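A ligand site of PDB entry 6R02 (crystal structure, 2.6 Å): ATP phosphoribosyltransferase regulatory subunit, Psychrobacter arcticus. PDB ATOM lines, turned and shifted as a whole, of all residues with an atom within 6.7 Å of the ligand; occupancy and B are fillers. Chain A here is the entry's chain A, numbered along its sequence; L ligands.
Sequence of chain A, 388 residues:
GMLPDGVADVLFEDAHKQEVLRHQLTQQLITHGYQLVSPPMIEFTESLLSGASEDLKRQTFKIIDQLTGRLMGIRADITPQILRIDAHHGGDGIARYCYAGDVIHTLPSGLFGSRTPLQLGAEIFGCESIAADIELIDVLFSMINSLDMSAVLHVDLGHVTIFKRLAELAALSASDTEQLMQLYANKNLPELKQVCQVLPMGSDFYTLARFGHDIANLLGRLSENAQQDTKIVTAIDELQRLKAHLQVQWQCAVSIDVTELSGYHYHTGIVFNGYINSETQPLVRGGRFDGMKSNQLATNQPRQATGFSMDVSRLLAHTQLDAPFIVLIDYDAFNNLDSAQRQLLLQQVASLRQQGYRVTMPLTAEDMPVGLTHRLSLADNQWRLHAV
OH of Tyr 266 is in hydrogen-bond range of N1 of the ligand, 3.1 Å away.
The guanidinium group (NE) of Arg 285 lies within salt-bridge range of an oxygen (O1) of the ligand, at 2.9 Å.
The side-chain hydroxyl (OG1) of Thr 79 is in hydrogen-bond range of a nitrogen (N1) of the ligand, 2.9 Å away.
The side-chain carboxylate (OE2) of Glu 123 sits at hydrogen-bond distance from a nitrogen (N3) of the ligand, 2.9 Å away.
A nitrogen (N2) of the ligand sits at hydrogen-bond distance from a ring nitrogen (NE2) of His 267 (3.4 Å).
The side-chain carboxylate (OD1) of Asp 77 lies within salt-bridge range of a nitrogen (N1) of the ligand (2.7 Å).
An oxygen (O2) of the ligand is in hydrogen-bond range of the side-chain amide nitrogen (NE2) of Gln 119.
OG of Ser 309 sits at hydrogen-bond distance from N1 of the ligand (3.2 Å).
O of Ala 122 is in hydrogen-bond range of N of Phe 308 (3.0 Å).
The side-chain carboxylate (OE1) of Glu 123 sits at hydrogen-bond distance from the side-chain hydroxyl (OG1) of Thr 79 (2.8 Å).
The backbone NH (N) of Ile 78 is in hydrogen-bond range of the side-chain amide oxygen (OE1) of Gln 119 (2.8 Å).
The side-chain hydroxyl of Thr 306 is in hydrogen-bond range of the backbone carbonyl oxygen of Gly 287, at 3.4 Å.
The backbone NH (N) of Ser 309 is in hydrogen-bond range of the backbone carbonyl oxygen (O) of Arg 285 (2.8 Å).
The side-chain carboxylate (OD2) of Asp 77 lies within hydrogen-bond range of the side-chain hydroxyl (OH) of Tyr 266 (2.7 Å).
OG1 of Thr 79 sits at hydrogen-bond distance from OH of Tyr 99, at 3.3 Å.
OH of Tyr 99 lies within hydrogen-bond range of O of Phe 308.
Tyr 264 touches the ligand.
CA of Gly 286 touches N2 of the ligand (3.9 Å).
Gly 287 touches the ligand.
CE1 of Phe 289 touches N3 of the ligand, 3.7 Å away.
C of Gly 307 touches N3 of the ligand, 3.3 Å away.
Phe 308 touches the ligand.
Hydrophobic or aromatic side chains that line the ligand: Tyr 264 and Phe 289.
Along chain A the residues within 4 Å of the ligand span positions 77 to 309.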
ATOM      1  N   ALA A  76       1.356  -8.697  31.623  1.00  0.00           N
ATOM      2  CA  ALA A  76       1.148  -7.562  30.688  1.00  0.00           C
ATOM      3  C   ALA A  76       0.357  -8.053  29.468  1.00  0.00           C
ATOM      4  O   ALA A  76      -0.047  -7.210  28.654  1.00  0.00           O
ATOM      5  CB  ALA A  76       2.473  -7.008  30.278  1.00  0.00           C
ATOM      6  N   ASP A  77       0.135  -9.375  29.378  1.00  0.00           N
ATOM      7  CA  ASP A  77      -0.495 -10.039  28.222  1.00  0.00           C
ATOM      8  C   ASP A  77      -0.974 -11.434  28.651  1.00  0.00           C
ATOM      9  O   ASP A  77      -0.206 -12.132  29.348  1.00  0.00           O
ATOM     10  CB  ASP A  77       0.487 -10.104  27.050  1.00  0.00           C
ATOM     11  CG  ASP A  77      -0.173 -10.451  25.730  1.00  0.00           C
ATOM     12  OD1 ASP A  77      -1.294  -9.982  25.468  1.00  0.00           O
ATOM     13  OD2 ASP A  77       0.451 -11.184  24.969  1.00  0.00           O
ATOM     14  N   ILE A  78      -2.183 -11.822  28.226  1.00  0.00           N
ATOM     15  CA  ILE A  78      -2.864 -13.089  28.624  1.00  0.00           C
ATOM     16  C   ILE A  78      -2.493 -14.208  27.638  1.00  0.00           C
ATOM     17  O   ILE A  78      -2.458 -15.376  28.061  1.00  0.00           O
ATOM     18  CB  ILE A  78      -4.386 -12.869  28.741  1.00  0.00           C
ATOM     19  CG1 ILE A  78      -4.719 -11.855  29.837  1.00  0.00           C
ATOM     20  CG2 ILE A  78      -5.126 -14.172  28.954  1.00  0.00           C
ATOM     21  CD1 ILE A  78      -6.076 -11.227  29.733  1.00  0.00           C
ATOM     22  N   THR A  79      -2.232 -13.865  26.374  1.00  0.00           N
ATOM     23  CA  THR A  79      -2.007 -14.831  25.268  1.00  0.00           C
ATOM     24  C   THR A  79      -1.004 -15.910  25.702  1.00  0.00           C
ATOM     25  O   THR A  79      -1.295 -17.102  25.559  1.00  0.00           O
ATOM     26  CB  THR A  79      -1.615 -14.105  23.977  1.00  0.00           C
ATOM     27  OG1 THR A  79      -2.703 -13.287  23.571  1.00  0.00           O
ATOM     28  CG2 THR A  79      -1.262 -15.044  22.847  1.00  0.00           C
ATOM     29  N   PRO A  80       0.182 -15.558  26.247  1.00  0.00           N
ATOM     30  CA  PRO A  80       1.112 -16.569  26.770  1.00  0.00           C
ATOM     31  C   PRO A  80       0.509 -17.514  27.821  1.00  0.00           C
ATOM     32  O   PRO A  80       0.951 -18.649  27.903  1.00  0.00           O
ATOM     33  CB  PRO A  80       2.239 -15.739  27.401  1.00  0.00           C
ATOM     34  CG  PRO A  80       2.228 -14.465  26.589  1.00  0.00           C
ATOM     35  CD  PRO A  80       0.758 -14.197  26.313  1.00  0.00           C
ATOM     36  N   TYR A  99     -11.027 -14.906  26.784  1.00  0.00           N
ATOM     37  CA  TYR A  99     -10.571 -14.395  28.100  1.00  0.00           C
ATOM     38  C   TYR A  99     -10.906 -12.911  28.182  1.00  0.00           C
ATOM     39  O   TYR A  99     -10.958 -12.233  27.140  1.00  0.00           O
ATOM     40  CB  TYR A  99      -9.076 -14.646  28.269  1.00  0.00           C
ATOM     41  CG  TYR A  99      -8.230 -14.143  27.125  1.00  0.00           C
ATOM     42  CD1 TYR A  99      -7.849 -12.818  27.049  1.00  0.00           C
ATOM     43  CD2 TYR A  99      -7.837 -15.000  26.112  1.00  0.00           C
ATOM     44  CE1 TYR A  99      -7.101 -12.349  25.982  1.00  0.00           C
ATOM     45  CE2 TYR A  99      -7.080 -14.543  25.043  1.00  0.00           C
ATOM     46  CZ  TYR A  99      -6.714 -13.215  24.982  1.00  0.00           C
ATOM     47  OH  TYR A  99      -5.956 -12.759  23.928  1.00  0.00           O
ATOM     48  N   GLN A 119      -7.938  -6.317  29.038  1.00  0.00           N
ATOM     49  CA  GLN A 119      -7.627  -7.127  27.832  1.00  0.00           C
ATOM     50  C   GLN A 119      -8.706  -8.198  27.670  1.00  0.00           C
ATOM     51  O   GLN A 119      -8.893  -9.004  28.603  1.00  0.00           O
ATOM     52  CB  GLN A 119      -6.237  -7.765  27.931  1.00  0.00           C
ATOM     53  CG  GLN A 119      -5.799  -8.513  26.692  1.00  0.00           C
ATOM     54  CD  GLN A 119      -4.373  -8.996  26.768  1.00  0.00           C
ATOM     55  OE1 GLN A 119      -4.055  -9.940  27.482  1.00  0.00           O
ATOM     56  NE2 GLN A 119      -3.505  -8.386  25.962  1.00  0.00           N
ATOM     57  N   GLY A 121     -10.095 -11.046  24.530  1.00  0.00           N
ATOM     58  CA  GLY A 121      -9.566 -11.681  23.313  1.00  0.00           C
ATOM     59  C   GLY A 121     -10.021 -13.107  23.102  1.00  0.00           C
ATOM     60  O   GLY A 121     -10.679 -13.685  23.998  1.00  0.00           O
ATOM     61  N   ALA A 122      -9.682 -13.648  21.926  1.00  0.00           N
ATOM     62  CA  ALA A 122      -9.927 -15.041  21.489  1.00  0.00           C
ATOM     63  C   ALA A 122      -8.663 -15.605  20.829  1.00  0.00           C
ATOM     64  O   ALA A 122      -7.908 -14.820  20.220  1.00  0.00           O
ATOM     65  CB  ALA A 122     -11.102 -15.081  20.544  1.00  0.00           C
ATOM     66  N   GLU A 123      -8.441 -16.913  20.981  1.00  0.00           N
ATOM     67  CA  GLU A 123      -7.329 -17.660  20.338  1.00  0.00           C
ATOM     68  C   GLU A 123      -7.903 -18.936  19.717  1.00  0.00           C
ATOM     69  O   GLU A 123      -8.728 -19.589  20.382  1.00  0.00           O
ATOM     70  CB  GLU A 123      -6.256 -18.045  21.359  1.00  0.00           C
ATOM     71  CG  GLU A 123      -5.923 -16.948  22.360  1.00  0.00           C
ATOM     72  CD  GLU A 123      -5.078 -15.808  21.831  1.00  0.00           C
ATOM     73  OE1 GLU A 123      -4.839 -14.837  22.586  1.00  0.00           O
ATOM     74  OE2 GLU A 123      -4.635 -15.892  20.685  1.00  0.00           O
ATOM     75  N   GLY A 263       3.753  -4.850  16.947  1.00  0.00           N
ATOM     76  CA  GLY A 263       3.089  -5.849  17.809  1.00  0.00           C
ATOM     77  C   GLY A 263       4.101  -6.716  18.540  1.00  0.00           C
ATOM     78  O   GLY A 263       5.306  -6.562  18.269  1.00  0.00           O
ATOM     79  N   TYR A 264       3.638  -7.567  19.460  1.00  0.00           N
ATOM     80  CA  TYR A 264       4.509  -8.427  20.300  1.00  0.00           C
ATOM     81  C   TYR A 264       5.276  -9.394  19.388  1.00  0.00           C
ATOM     82  O   TYR A 264       4.651 -10.032  18.560  1.00  0.00           O
ATOM     83  CB  TYR A 264       3.689  -9.207  21.341  1.00  0.00           C
ATOM     84  CG  TYR A 264       3.200  -8.388  22.496  1.00  0.00           C
ATOM     85  CD1 TYR A 264       4.081  -7.610  23.239  1.00  0.00           C
ATOM     86  CD2 TYR A 264       1.859  -8.386  22.856  1.00  0.00           C
ATOM     87  CE1 TYR A 264       3.642  -6.842  24.309  1.00  0.00           C
ATOM     88  CE2 TYR A 264       1.408  -7.637  23.931  1.00  0.00           C
ATOM     89  CZ  TYR A 264       2.303  -6.862  24.658  1.00  0.00           C
ATOM     90  OH  TYR A 264       1.883  -6.104  25.717  1.00  0.00           O
ATOM     91  N   TYR A 266       6.396 -12.251  19.453  1.00  0.00           N
ATOM     92  CA  TYR A 266       6.081 -13.703  19.445  1.00  0.00           C
ATOM     93  C   TYR A 266       5.255 -14.059  18.185  1.00  0.00           C
ATOM     94  O   TYR A 266       4.985 -15.262  17.960  1.00  0.00           O
ATOM     95  CB  TYR A 266       5.433 -14.192  20.757  1.00  0.00           C
ATOM     96  CG  TYR A 266       4.145 -13.543  21.202  1.00  0.00           C
ATOM     97  CD1 TYR A 266       2.970 -13.737  20.500  1.00  0.00           C
ATOM     98  CD2 TYR A 266       4.080 -12.766  22.355  1.00  0.00           C
ATOM     99  CE1 TYR A 266       1.782 -13.124  20.871  1.00  0.00           C
ATOM    100  CE2 TYR A 266       2.891 -12.170  22.760  1.00  0.00           C
ATOM    101  CZ  TYR A 266       1.751 -12.326  22.003  1.00  0.00           C
ATOM    102  OH  TYR A 266       0.567 -11.755  22.375  1.00  0.00           O
ATOM    103  N   HIS A 267       4.876 -13.044  17.395  1.00  0.00           N
ATOM    104  CA  HIS A 267       4.092 -13.183  16.127  1.00  0.00           C
ATOM    105  C   HIS A 267       4.987 -13.849  15.074  1.00  0.00           C
ATOM    106  O   HIS A 267       6.160 -13.460  14.950  1.00  0.00           O
ATOM    107  CB  HIS A 267       3.570 -11.815  15.664  1.00  0.00           C
ATOM    108  CG  HIS A 267       2.476 -11.266  16.534  1.00  0.00           C
ATOM    109  ND1 HIS A 267       1.684 -10.191  16.163  1.00  0.00           N
ATOM    110  CD2 HIS A 267       2.012 -11.669  17.738  1.00  0.00           C
ATOM    111  CE1 HIS A 267       0.808  -9.949  17.121  1.00  0.00           C
ATOM    112  NE2 HIS A 267       0.992 -10.844  18.095  1.00  0.00           N
ATOM    113  N   VAL A 284      -7.655  -3.044  18.580  1.00  0.00           N
ATOM    114  CA  VAL A 284      -7.493  -4.527  18.417  1.00  0.00           C
ATOM    115  C   VAL A 284      -6.104  -4.818  17.850  1.00  0.00           C
ATOM    116  O   VAL A 284      -5.703  -4.139  16.903  1.00  0.00           O
ATOM    117  CB  VAL A 284      -8.587  -5.126  17.501  1.00  0.00           C
ATOM    118  CG1 VAL A 284      -8.775  -6.602  17.800  1.00  0.00           C
ATOM    119  CG2 VAL A 284      -9.899  -4.374  17.612  1.00  0.00           C
ATOM    120  N   ARG A 285      -5.422  -5.808  18.432  1.00  0.00           N
ATOM    121  CA  ARG A 285      -4.148  -6.386  17.942  1.00  0.00           C
ATOM    122  C   ARG A 285      -4.327  -7.906  17.845  1.00  0.00           C
ATOM    123  O   ARG A 285      -4.841  -8.479  18.784  1.00  0.00           O
ATOM    124  CB  ARG A 285      -2.997  -6.021  18.866  1.00  0.00           C
ATOM    125  CG  ARG A 285      -2.471  -4.606  18.651  1.00  0.00           C
ATOM    126  CD  ARG A 285      -2.020  -3.881  19.907  1.00  0.00           C
ATOM    127  NE  ARG A 285      -1.080  -4.613  20.752  1.00  0.00           N
ATOM    128  CZ  ARG A 285       0.258  -4.541  20.677  1.00  0.00           C
ATOM    129  NH1 ARG A 285       0.988  -5.239  21.528  1.00  0.00           N
ATOM    130  NH2 ARG A 285       0.850  -3.786  19.765  1.00  0.00           N
ATOM    131  N   GLY A 286      -3.906  -8.510  16.737  1.00  0.00           N
ATOM    132  CA  GLY A 286      -4.014  -9.958  16.507  1.00  0.00           C
ATOM    133  C   GLY A 286      -2.955 -10.458  15.548  1.00  0.00           C
ATOM    134  O   GLY A 286      -2.295  -9.626  14.899  1.00  0.00           O
ATOM    135  N   GLY A 287      -2.803 -11.789  15.466  1.00  0.00           N
ATOM    136  CA  GLY A 287      -1.911 -12.450  14.493  1.00  0.00           C
ATOM    137  C   GLY A 287      -1.599 -13.885  14.861  1.00  0.00           C
ATOM    138  O   GLY A 287      -2.058 -14.346  15.904  1.00  0.00           O
ATOM    139  N   ARG A 288      -0.817 -14.547  14.015  1.00  0.00           N
ATOM    140  CA  ARG A 288      -0.317 -15.936  14.189  1.00  0.00           C
ATOM    141  C   ARG A 288       0.808 -15.964  15.237  1.00  0.00           C
ATOM    142  O   ARG A 288       1.541 -14.995  15.305  1.00  0.00           O
ATOM    143  CB  ARG A 288       0.186 -16.482  12.851  1.00  0.00           C
ATOM    144  CG  ARG A 288      -0.932 -16.894  11.894  1.00  0.00           C
ATOM    145  CD  ARG A 288      -1.236 -18.378  12.018  1.00  0.00           C
ATOM    146  NE  ARG A 288      -2.522 -18.744  11.452  1.00  0.00           N
ATOM    147  CZ  ARG A 288      -3.096 -19.936  11.585  1.00  0.00           C
ATOM    148  NH1 ARG A 288      -2.487 -20.894  12.266  1.00  0.00           N
ATOM    149  NH2 ARG A 288      -4.280 -20.171  11.036  1.00  0.00           N
ATOM    150  N   PHE A 289       0.915 -17.044  16.003  1.00  0.00           N
ATOM    151  CA  PHE A 289       2.006 -17.318  16.981  1.00  0.00           C
ATOM    152  C   PHE A 289       2.153 -18.848  17.092  1.00  0.00           C
ATOM    153  O   PHE A 289       1.344 -19.538  16.463  1.00  0.00           O
ATOM    154  CB  PHE A 289       1.749 -16.583  18.300  1.00  0.00           C
ATOM    155  CG  PHE A 289       0.494 -16.977  19.036  1.00  0.00           C
ATOM    156  CD1 PHE A 289      -0.750 -16.509  18.629  1.00  0.00           C
ATOM    157  CD2 PHE A 289       0.551 -17.800  20.149  1.00  0.00           C
ATOM    158  CE1 PHE A 289      -1.903 -16.857  19.296  1.00  0.00           C
ATOM    159  CE2 PHE A 289      -0.605 -18.144  20.825  1.00  0.00           C
ATOM    160  CZ  PHE A 289      -1.825 -17.673  20.401  1.00  0.00           C
ATOM    161  N   ALA A 305      -1.289 -21.494  16.124  1.00  0.00           N
ATOM    162  CA  ALA A 305      -2.065 -20.564  16.981  1.00  0.00           C
ATOM    163  C   ALA A 305      -2.261 -19.223  16.264  1.00  0.00           C
ATOM    164  O   ALA A 305      -1.323 -18.745  15.632  1.00  0.00           O
ATOM    165  CB  ALA A 305      -1.370 -20.370  18.303  1.00  0.00           C
ATOM    166  N   THR A 306      -3.463 -18.659  16.378  1.00  0.00           N
ATOM    167  CA  THR A 306      -3.815 -17.288  15.933  1.00  0.00           C
ATOM    168  C   THR A 306      -4.893 -16.761  16.870  1.00  0.00           C
ATOM    169  O   THR A 306      -5.650 -17.579  17.423  1.00  0.00           O
ATOM    170  CB  THR A 306      -4.225 -17.279  14.454  1.00  0.00           C
ATOM    171  OG1 THR A 306      -4.464 -15.929  14.066  1.00  0.00           O
ATOM    172  CG2 THR A 306      -5.449 -18.127  14.183  1.00  0.00           C
ATOM    173  N   GLY A 307      -4.943 -15.436  17.069  1.00  0.00           N
ATOM    174  CA  GLY A 307      -5.898 -14.791  17.988  1.00  0.00           C
ATOM    175  C   GLY A 307      -5.853 -13.288  17.896  1.00  0.00           C
ATOM    176  O   GLY A 307      -5.073 -12.778  17.062  1.00  0.00           O
ATOM    177  N   PHE A 308      -6.673 -12.606  18.691  1.00  0.00           N
ATOM    178  CA  PHE A 308      -6.696 -11.130  18.853  1.00  0.00           C
ATOM    179  C   PHE A 308      -6.978 -10.772  20.311  1.00  0.00           C
ATOM    180  O   PHE A 308      -7.501 -11.624  21.051  1.00  0.00           O
ATOM    181  CB  PHE A 308      -7.723 -10.499  17.908  1.00  0.00           C
ATOM    182  CG  PHE A 308      -9.152 -10.856  18.215  1.00  0.00           C
ATOM    183  CD1 PHE A 308      -9.865 -10.153  19.175  1.00  0.00           C
ATOM    184  CD2 PHE A 308      -9.777 -11.907  17.569  1.00  0.00           C
ATOM    185  CE1 PHE A 308     -11.171 -10.492  19.472  1.00  0.00           C
ATOM    186  CE2 PHE A 308     -11.083 -12.246  17.866  1.00  0.00           C
ATOM    187  CZ  PHE A 308     -11.790 -11.535  18.812  1.00  0.00           C
ATOM    188  N   SER A 309      -6.625  -9.548  20.704  1.00  0.00           N
ATOM    189  CA  SER A 309      -6.935  -8.926  22.004  1.00  0.00           C
ATOM    190  C   SER A 309      -7.385  -7.489  21.774  1.00  0.00           C
ATOM    191  O   SER A 309      -6.947  -6.896  20.782  1.00  0.00           O
ATOM    192  CB  SER A 309      -5.748  -8.973  22.905  1.00  0.00           C
ATOM    193  OG  SER A 309      -5.427 -10.317  23.250  1.00  0.00           O
ATOM    194  N   MET A 310      -8.227  -6.948  22.652  1.00  0.00           N
ATOM    195  CA  MET A 310      -8.630  -5.524  22.630  1.00  0.00           C
ATOM    196  C   MET A 310      -8.761  -5.017  24.066  1.00  0.00           C
ATOM    197  O   MET A 310      -9.054  -5.829  24.960  1.00  0.00           O
ATOM    198  CB  MET A 310      -9.948  -5.313  21.876  1.00  0.00           C
ATOM    199  CG  MET A 310     -11.165  -5.915  22.562  1.00  0.00           C
ATOM    200  SD  MET A 310     -12.707  -5.442  21.742  1.00  0.00           S
ATOM    201  CE  MET A 310     -13.186  -7.023  21.049  1.00  0.00           C
HETATM  202  N1  LIG L   1      -2.225 -10.446  22.966  1.00  0.00           N
HETATM  203  C1  LIG L   1      -1.849  -9.646  21.760  1.00  0.00           C
HETATM  204  C2  LIG L   1      -1.797  -8.154  22.125  1.00  0.00           C
HETATM  205  O1  LIG L   1      -1.121  -7.378  21.465  1.00  0.00           O
HETATM  206  C3  LIG L   1      -2.816  -9.940  20.603  1.00  0.00           C
HETATM  207  C4  LIG L   1      -2.848 -11.374  20.202  1.00  0.00           C
HETATM  208  N2  LIG L   1      -1.996 -11.893  19.255  1.00  0.00           N
HETATM  209  C5  LIG L   1      -3.611 -12.406  20.630  1.00  0.00           C
HETATM  210  C6  LIG L   1      -2.233 -13.179  19.114  1.00  0.00           C
HETATM  211  N3  LIG L   1      -3.225 -13.513  19.946  1.00  0.00           N
HETATM  212  O2  LIG L   1      -2.433  -7.713  23.080  1.00  0.00           O
